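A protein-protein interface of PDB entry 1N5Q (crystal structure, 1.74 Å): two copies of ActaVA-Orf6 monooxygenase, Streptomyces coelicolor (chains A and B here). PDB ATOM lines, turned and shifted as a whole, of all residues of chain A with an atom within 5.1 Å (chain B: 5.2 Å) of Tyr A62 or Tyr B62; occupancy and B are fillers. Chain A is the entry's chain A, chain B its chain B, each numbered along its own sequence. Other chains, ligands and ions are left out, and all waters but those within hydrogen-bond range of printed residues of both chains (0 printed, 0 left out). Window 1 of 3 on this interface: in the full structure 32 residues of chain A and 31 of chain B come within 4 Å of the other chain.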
ATOM      1  N   VAL A   3       7.879 -26.046  23.365  1.00  0.00           N
ATOM      2  CA  VAL A   3       7.498 -25.902  21.958  1.00  0.00           C
ATOM      3  C   VAL A   3       8.642 -26.063  20.981  1.00  0.00           C
ATOM      4  O   VAL A   3       8.373 -26.424  19.845  1.00  0.00           O
ATOM      5  CB  VAL A   3       6.791 -24.542  21.773  1.00  0.00           C
ATOM      6  CG1 VAL A   3       5.461 -24.591  22.547  1.00  0.00           C
ATOM      7  CG2 VAL A   3       7.648 -23.380  22.265  1.00  0.00           C
ATOM      8  N   VAL A  11       3.647 -32.318  14.119  1.00  0.00           N
ATOM      9  CA  VAL A  11       2.539 -31.673  14.846  1.00  0.00           C
ATOM     10  C   VAL A  11       1.240 -31.765  14.066  1.00  0.00           C
ATOM     11  O   VAL A  11       1.233 -31.575  12.832  1.00  0.00           O
ATOM     12  CB  VAL A  11       2.872 -30.184  15.081  1.00  0.00           C
ATOM     13  CG1 VAL A  11       1.677 -29.343  15.558  1.00  0.00           C
ATOM     14  CG2 VAL A  11       3.965 -30.035  16.151  1.00  0.00           C
ATOM     15  N   ALA A  12       0.118 -31.977  14.782  1.00  0.00           N
ATOM     16  CA  ALA A  12      -1.174 -31.923  14.110  1.00  0.00           C
ATOM     17  C   ALA A  12      -1.993 -30.795  14.741  1.00  0.00           C
ATOM     18  O   ALA A  12      -1.963 -30.764  15.968  1.00  0.00           O
ATOM     19  CB  ALA A  12      -1.919 -33.255  14.247  1.00  0.00           C
ATOM     20  N   VAL A  13      -2.638 -29.925  13.966  1.00  0.00           N
ATOM     21  CA  VAL A  13      -3.467 -28.863  14.554  1.00  0.00           C
ATOM     22  C   VAL A  13      -4.889 -29.181  14.073  1.00  0.00           C
ATOM     23  O   VAL A  13      -5.160 -29.152  12.866  1.00  0.00           O
ATOM     24  CB  VAL A  13      -3.049 -27.434  14.162  1.00  0.00           C
ATOM     25  CG1 VAL A  13      -4.114 -26.441  14.721  1.00  0.00           C
ATOM     26  CG2 VAL A  13      -1.680 -27.112  14.712  1.00  0.00           C
ATOM     27  N   SER A  47       2.123 -34.631  23.421  1.00  0.00           N
ATOM     28  CA  SER A  47       1.116 -33.817  24.112  1.00  0.00           C
ATOM     29  C   SER A  47      -0.052 -33.490  23.176  1.00  0.00           C
ATOM     30  O   SER A  47       0.026 -33.630  21.954  1.00  0.00           O
ATOM     31  CB  SER A  47       1.655 -32.463  24.560  1.00  0.00           C
ATOM     32  OG  SER A  47       1.922 -31.661  23.380  1.00  0.00           O
ATOM     33  N   ALA A  48      -1.161 -33.171  23.840  1.00  0.00           N
ATOM     34  CA  ALA A  48      -2.344 -32.707  23.081  1.00  0.00           C
ATOM     35  C   ALA A  48      -2.934 -31.580  23.927  1.00  0.00           C
ATOM     36  O   ALA A  48      -3.372 -31.836  25.062  1.00  0.00           O
ATOM     37  CB  ALA A  48      -3.354 -33.764  22.757  1.00  0.00           C
ATOM     38  N   THR A  49      -2.893 -30.346  23.409  1.00  0.00           N
ATOM     39  CA  THR A  49      -3.345 -29.185  24.166  1.00  0.00           C
ATOM     40  C   THR A  49      -4.618 -28.617  23.549  1.00  0.00           C
ATOM     41  O   THR A  49      -4.555 -28.241  22.363  1.00  0.00           O
ATOM     42  CB  THR A  49      -2.311 -28.045  24.267  1.00  0.00           C
ATOM     43  OG1 THR A  49      -1.154 -28.571  24.924  1.00  0.00           O
ATOM     44  CG2 THR A  49      -2.763 -26.829  25.082  1.00  0.00           C
ATOM     45  N   HIS A  51      -7.627 -25.825  23.240  1.00  0.00           N
ATOM     46  CA  HIS A  51      -7.846 -24.402  23.518  1.00  0.00           C
ATOM     47  C   HIS A  51      -9.213 -23.970  23.013  1.00  0.00           C
ATOM     48  O   HIS A  51      -9.773 -24.539  22.074  1.00  0.00           O
ATOM     49  CB  HIS A  51      -6.851 -23.619  22.634  1.00  0.00           C
ATOM     50  CG  HIS A  51      -5.415 -24.000  22.605  1.00  0.00           C
ATOM     51  ND1 HIS A  51      -4.976 -25.159  21.981  1.00  0.00           N
ATOM     52  CD2 HIS A  51      -4.295 -23.328  23.043  1.00  0.00           C
ATOM     53  CE1 HIS A  51      -3.638 -25.204  22.022  1.00  0.00           C
ATOM     54  NE2 HIS A  51      -3.241 -24.115  22.666  1.00  0.00           N
ATOM     55  N   VAL A  60      -9.464 -25.776  19.514  1.00  0.00           N
ATOM     56  CA  VAL A  60      -8.294 -26.155  18.675  1.00  0.00           C
ATOM     57  C   VAL A  60      -7.364 -27.066  19.504  1.00  0.00           C
ATOM     58  O   VAL A  60      -7.025 -26.659  20.599  1.00  0.00           O
ATOM     59  CB  VAL A  60      -7.574 -24.867  18.250  1.00  0.00           C
ATOM     60  CG1 VAL A  60      -6.335 -25.219  17.455  1.00  0.00           C
ATOM     61  CG2 VAL A  60      -8.541 -23.994  17.404  1.00  0.00           C
ATOM     62  N   ASN A  61      -6.971 -28.193  18.900  1.00  0.00           N
ATOM     63  CA  ASN A  61      -5.978 -29.062  19.523  1.00  0.00           C
ATOM     64  C   ASN A  61      -4.595 -28.907  18.847  1.00  0.00           C
ATOM     65  O   ASN A  61      -4.577 -29.193  17.656  1.00  0.00           O
ATOM     66  CB  ASN A  61      -6.467 -30.485  19.408  1.00  0.00           C
ATOM     67  CG  ASN A  61      -5.528 -31.608  19.832  1.00  0.00           C
ATOM     68  OD1 ASN A  61      -4.532 -31.294  20.482  1.00  0.00           O
ATOM     69  ND2 ASN A  61      -5.830 -32.835  19.444  1.00  0.00           N
ATOM     70  N   TYR A  62      -3.590 -28.538  19.627  1.00  0.00           N
ATOM     71  CA  TYR A  62      -2.197 -28.512  19.132  1.00  0.00           C
ATOM     72  C   TYR A  62      -1.549 -29.796  19.696  1.00  0.00           C
ATOM     73  O   TYR A  62      -1.494 -29.912  20.908  1.00  0.00           O
ATOM     74  CB  TYR A  62      -1.462 -27.275  19.629  1.00  0.00           C
ATOM     75  CG  TYR A  62      -0.015 -27.137  19.210  1.00  0.00           C
ATOM     76  CD1 TYR A  62       0.319 -26.567  17.984  1.00  0.00           C
ATOM     77  CD2 TYR A  62       0.998 -27.536  20.061  1.00  0.00           C
ATOM     78  CE1 TYR A  62       1.623 -26.389  17.588  1.00  0.00           C
ATOM     79  CE2 TYR A  62       2.336 -27.402  19.690  1.00  0.00           C
ATOM     80  CZ  TYR A  62       2.625 -26.838  18.461  1.00  0.00           C
ATOM     81  OH  TYR A  62       3.956 -26.704  18.095  1.00  0.00           O
ATOM     82  N   ALA A  63      -1.197 -30.718  18.821  1.00  0.00           N
ATOM     83  CA  ALA A  63      -0.689 -32.004  19.376  1.00  0.00           C
ATOM     84  C   ALA A  63       0.738 -32.258  18.913  1.00  0.00           C
ATOM     85  O   ALA A  63       0.962 -32.116  17.707  1.00  0.00           O
ATOM     86  CB  ALA A  63      -1.593 -33.093  18.882  1.00  0.00           C
ATOM     87  N   GLN A  64       1.621 -32.537  19.862  1.00  0.00           N
ATOM     88  CA  GLN A  64       3.024 -32.829  19.509  1.00  0.00           C
ATOM     89  C   GLN A  64       3.352 -34.297  19.489  1.00  0.00           C
ATOM     90  O   GLN A  64       2.889 -35.095  20.335  1.00  0.00           O
ATOM     91  CB  GLN A  64       3.950 -32.222  20.635  1.00  0.00           C
ATOM     92  CG  GLN A  64       3.930 -30.692  20.699  1.00  0.00           C
ATOM     93  CD  GLN A  64       4.614 -30.259  21.999  1.00  0.00           C
ATOM     94  OE1 GLN A  64       4.451 -30.850  23.082  1.00  0.00           O
ATOM     95  NE2 GLN A  64       5.447 -29.254  21.888  1.00  0.00           N
ATOM     96  N   VAL B   3       3.884 -26.834  26.841  1.00  0.00           N
ATOM     97  CA  VAL B   3       2.569 -26.481  26.310  1.00  0.00           C
ATOM     98  C   VAL B   3       1.534 -26.206  27.378  1.00  0.00           C
ATOM     99  O   VAL B   3       0.567 -25.449  27.127  1.00  0.00           O
ATOM    100  CB  VAL B   3       2.002 -27.518  25.307  1.00  0.00           C
ATOM    101  CG1 VAL B   3       2.877 -27.424  24.042  1.00  0.00           C
ATOM    102  CG2 VAL B   3       1.927 -28.922  25.828  1.00  0.00           C
ATOM    103  N   VAL B  11      -2.915 -17.665  23.308  1.00  0.00           N
ATOM    104  CA  VAL B  11      -2.218 -18.278  22.198  1.00  0.00           C
ATOM    105  C   VAL B  11      -2.710 -17.699  20.852  1.00  0.00           C
ATOM    106  O   VAL B  11      -3.914 -17.531  20.716  1.00  0.00           O
ATOM    107  CB  VAL B  11      -2.482 -19.804  22.184  1.00  0.00           C
ATOM    108  CG1 VAL B  11      -2.041 -20.453  20.847  1.00  0.00           C
ATOM    109  CG2 VAL B  11      -1.656 -20.486  23.295  1.00  0.00           C
ATOM    110  N   ALA B  12      -1.762 -17.386  19.953  1.00  0.00           N
ATOM    111  CA  ALA B  12      -2.262 -16.934  18.592  1.00  0.00           C
ATOM    112  C   ALA B  12      -1.763 -18.010  17.646  1.00  0.00           C
ATOM    113  O   ALA B  12      -0.602 -18.501  17.750  1.00  0.00           O
ATOM    114  CB  ALA B  12      -1.695 -15.614  18.218  1.00  0.00           C
ATOM    115  N   VAL B  13      -2.579 -18.455  16.696  1.00  0.00           N
ATOM    116  CA  VAL B  13      -2.175 -19.419  15.681  1.00  0.00           C
ATOM    117  C   VAL B  13      -2.397 -18.707  14.329  1.00  0.00           C
ATOM    118  O   VAL B  13      -3.514 -18.350  14.001  1.00  0.00           O
ATOM    119  CB  VAL B  13      -2.991 -20.709  15.773  1.00  0.00           C
ATOM    120  CG1 VAL B  13      -2.543 -21.607  14.627  1.00  0.00           C
ATOM    121  CG2 VAL B  13      -2.748 -21.437  17.118  1.00  0.00           C
ATOM    122  N   VAL B  14      -1.297 -18.419  13.650  1.00  0.00           N
ATOM    123  CA  VAL B  14      -1.364 -17.577  12.439  1.00  0.00           C
ATOM    124  C   VAL B  14      -0.940 -18.441  11.260  1.00  0.00           C
ATOM    125  O   VAL B  14       0.142 -19.019  11.274  1.00  0.00           O
ATOM    126  CB  VAL B  14      -0.391 -16.392  12.584  1.00  0.00           C
ATOM    127  CG1 VAL B  14      -0.551 -15.483  11.346  1.00  0.00           C
ATOM    128  CG2 VAL B  14      -0.635 -15.584  13.856  1.00  0.00           C
ATOM    129  N   SER B  47       6.742 -17.466  23.492  1.00  0.00           N
ATOM    130  CA  SER B  47       7.348 -18.259  22.436  1.00  0.00           C
ATOM    131  C   SER B  47       6.582 -18.096  21.112  1.00  0.00           C
ATOM    132  O   SER B  47       5.430 -17.612  21.105  1.00  0.00           O
ATOM    133  CB  SER B  47       7.300 -19.779  22.733  1.00  0.00           C
ATOM    134  OG  SER B  47       5.915 -20.206  22.551  1.00  0.00           O
ATOM    135  N   ALA B  48       7.343 -18.297  20.021  1.00  0.00           N
ATOM    136  CA  ALA B  48       6.697 -18.300  18.691  1.00  0.00           C
ATOM    137  C   ALA B  48       7.340 -19.453  17.943  1.00  0.00           C
ATOM    138  O   ALA B  48       8.583 -19.449  17.834  1.00  0.00           O
ATOM    139  CB  ALA B  48       6.821 -16.994  17.948  1.00  0.00           C
ATOM    140  N   THR B  49       6.591 -20.450  17.480  1.00  0.00           N
ATOM    141  CA  THR B  49       7.207 -21.591  16.794  1.00  0.00           C
ATOM    142  C   THR B  49       6.650 -21.637  15.390  1.00  0.00           C
ATOM    143  O   THR B  49       5.403 -21.666  15.237  1.00  0.00           O
ATOM    144  CB  THR B  49       6.918 -22.903  17.543  1.00  0.00           C
ATOM    145  OG1 THR B  49       7.435 -22.884  18.889  1.00  0.00           O
ATOM    146  CG2 THR B  49       7.551 -24.102  16.793  1.00  0.00           C
ATOM    147  N   HIS B  51       6.043 -23.484  11.739  1.00  0.00           N
ATOM    148  CA  HIS B  51       5.985 -24.816  11.222  1.00  0.00           C
ATOM    149  C   HIS B  51       5.712 -24.757   9.700  1.00  0.00           C
ATOM    150  O   HIS B  51       5.100 -23.808   9.235  1.00  0.00           O
ATOM    151  CB  HIS B  51       4.804 -25.656  11.762  1.00  0.00           C
ATOM    152  CG  HIS B  51       4.650 -25.607  13.267  1.00  0.00           C
ATOM    153  ND1 HIS B  51       4.287 -24.456  13.926  1.00  0.00           N
ATOM    154  CD2 HIS B  51       4.757 -26.579  14.187  1.00  0.00           C
ATOM    155  CE1 HIS B  51       4.226 -24.714  15.264  1.00  0.00           C
ATOM    156  NE2 HIS B  51       4.507 -25.992  15.422  1.00  0.00           N
ATOM    157  N   VAL B  60       2.710 -22.133   9.578  1.00  0.00           N
ATOM    158  CA  VAL B  60       1.828 -21.856  10.724  1.00  0.00           C
ATOM    159  C   VAL B  60       2.693 -21.441  11.921  1.00  0.00           C
ATOM    160  O   VAL B  60       3.628 -22.149  12.269  1.00  0.00           O
ATOM    161  CB  VAL B  60       1.060 -23.171  11.082  1.00  0.00           C
ATOM    162  CG1 VAL B  60       0.258 -22.946  12.371  1.00  0.00           C
ATOM    163  CG2 VAL B  60       0.136 -23.584   9.937  1.00  0.00           C
ATOM    164  N   ASN B  61       2.336 -20.324  12.561  1.00  0.00           N
ATOM    165  CA  ASN B  61       3.020 -19.854  13.780  1.00  0.00           C
ATOM    166  C   ASN B  61       2.091 -20.128  14.988  1.00  0.00           C
ATOM    167  O   ASN B  61       0.958 -19.643  14.985  1.00  0.00           O
ATOM    168  CB  ASN B  61       3.286 -18.350  13.650  1.00  0.00           C
ATOM    169  CG  ASN B  61       3.803 -17.687  14.935  1.00  0.00           C
ATOM    170  OD1 ASN B  61       4.209 -18.363  15.865  1.00  0.00           O
ATOM    171  ND2 ASN B  61       3.764 -16.368  15.007  1.00  0.00           N
ATOM    172  N   TYR B  62       2.579 -20.922  15.940  1.00  0.00           N
ATOM    173  CA  TYR B  62       1.895 -21.139  17.230  1.00  0.00           C
ATOM    174  C   TYR B  62       2.622 -20.249  18.229  1.00  0.00           C
ATOM    175  O   TYR B  62       3.821 -20.470  18.407  1.00  0.00           O
ATOM    176  CB  TYR B  62       1.972 -22.615  17.605  1.00  0.00           C
ATOM    177  CG  TYR B  62       1.373 -22.932  18.963  1.00  0.00           C
ATOM    178  CD1 TYR B  62       2.112 -22.924  20.129  1.00  0.00           C
ATOM    179  CD2 TYR B  62       0.005 -23.248  18.993  1.00  0.00           C
ATOM    180  CE1 TYR B  62       1.503 -23.252  21.360  1.00  0.00           C
ATOM    181  CE2 TYR B  62      -0.570 -23.572  20.224  1.00  0.00           C
ATOM    182  CZ  TYR B  62       0.162 -23.572  21.372  1.00  0.00           C
ATOM    183  OH  TYR B  62      -0.498 -23.932  22.573  1.00  0.00           O
ATOM    184  N   ALA B  63       1.968 -19.230  18.774  1.00  0.00           N
ATOM    185  CA  ALA B  63       2.713 -18.298  19.649  1.00  0.00           C
ATOM    186  C   ALA B  63       2.069 -18.270  21.041  1.00  0.00           C
ATOM    187  O   ALA B  63       0.845 -18.187  21.170  1.00  0.00           O
ATOM    188  CB  ALA B  63       2.638 -16.861  19.073  1.00  0.00           C
ATOM    189  N   GLN B  64       2.915 -18.328  22.065  1.00  0.00           N
ATOM    190  CA  GLN B  64       2.439 -18.325  23.445  1.00  0.00           C
ATOM    191  C   GLN B  64       2.699 -16.971  24.093  1.00  0.00           C
ATOM    192  O   GLN B  64       3.782 -16.436  23.906  1.00  0.00           O
ATOM    193  CB  GLN B  64       3.297 -19.334  24.231  1.00  0.00           C
ATOM    194  CG  GLN B  64       3.013 -20.813  23.870  1.00  0.00           C
ATOM    195  CD  GLN B  64       4.041 -21.702  24.546  1.00  0.00           C
ATOM    196  OE1 GLN B  64       5.268 -21.407  24.600  1.00  0.00           O
ATOM    197  NE2 GLN B  64       3.587 -22.822  25.093  1.00  0.00           N
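NE2 of His A51 is in hydrogen-bond range of OH of Tyr B62. The side-chain hydroxyl (OH) of Tyr A62 sits at hydrogen-bond distance from a ring nitrogen (NE2) of His B51 (2.8 Å).
The side-chain hydroxyl of Ser A47 is in hydrogen-bond range of the side-chain amide oxygen of Gln A64. The side-chain amide oxygen (OD1) of Asn A61 lies within hydrogen-bond range of the backbone NH (N) of Thr A49. The backbone carbonyl oxygen (O) of Tyr A62 is in hydrogen-bond range of the backbone NH (N) of Thr A49, at 2.9 Å. O of Val A60 is in hydrogen-bond range of N of His A51, at 2.8 Å. The backbone NH of Thr B49 is in hydrogen-bond range of the backbone carbonyl oxygen of Tyr B62 (2.9 Å). The backbone carbonyl oxygen of Val B60 sits at hydrogen-bond distance from the backbone NH of His B51.
CG2 of Val A3 touches OG of Ser B47 (3.6 Å). OG1 of Thr B49 touches CB of Val A3, 3.4 Å away. Val A3 touches Gln B64. Ser A47 touches Val B3 (OG to CG2, 3.7 Å). Thr A49 touches Val B3 (OG1 to CG2, 3.2 Å). CD2 of His A51 touches CG2 of Val B11 (3.9 Å). Tyr A62 touches Tyr B62 (CD1 to CD2, 3.5 Å). Gln A64 touches Val B3 (NE2 to CG1, 3.8 Å).
Of the printed residues of chain B, Tyr A62 touches His B51 and Tyr B62. Tyr B62 touches just these residues of chain A: His A51 and Tyr A62. Of the printed residues of chain A, Thr B49 touches Val A3 (3.4 Å). Printed residues of chain B within 4 Å of Ser A47: Val B3 (3.7 Å). Of the printed residues of chain A, Val B11 touches His A51 (3.9 Å). Of the printed residues of chain B, Val A3 touches Ser B47 (3.6 Å), Thr B49 (3.4 Å) and Gln B64 (3.6 Å). Val B60 touches none of the printed residues of chain A. The nearest residue of chain B that does not touch Tyr A62 is Val B3 (4.4 Å). The nearest residue of chain A that does not touch Tyr B62 is Val A3 (4.3 Å).
Printed residues of chain B that touch a printed residue of chain A: Val B3, Val B11, Ser B47, Thr B49, His B51, Tyr B62 and Gln B64. Hydrophobic or aromatic side chains of chain B within 4 Å of the printed part of chain A: Val B3, Val B11, His B51 and Tyr B62. Along chain B the printed residues that touch a printed residue of chain A span positions 3 to 64. Of the 13 printed residues of chain A, 6 touch a printed residue of chain B. Printed residues of chain A that touch a printed residue of chain B: Val A3, Ser A47, Thr A49, His A51, Tyr A62 and Gln A64. Hydrophobic or aromatic side chains of chain A that line the printed part of chain B: Val A3, His A51 and Tyr A62. Along chain A the printed residues that touch a printed residue of chain B span positions 3 to 64. Among the printed residues, 10 pairs touch across the chains. Among the printed residues, no Asp or Glu carboxylate lies within 4 Å of a Lys or Arg side-chain nitrogen of the other chain.
Val A3 touches Thr B49, and with the chains exchanged Thr A49 touches Val B3. His A51 touches Val B11, but with the chains exchanged Val A11 does not touch His B51 (4.1 Å). His A51 touches Tyr B62, and with the chains exchanged Tyr A62 touches His B51. Tyr B62 touches its own counterpart, Tyr A62. Positions printed for both chains: 3, 11, 12, 13, 47, 48, 49, 51, 60, 61, 62, 63 and 64. Of the 10 pairs that touch across the chains among the printed residues, 9 have their exchanged pair printed and touching as well.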
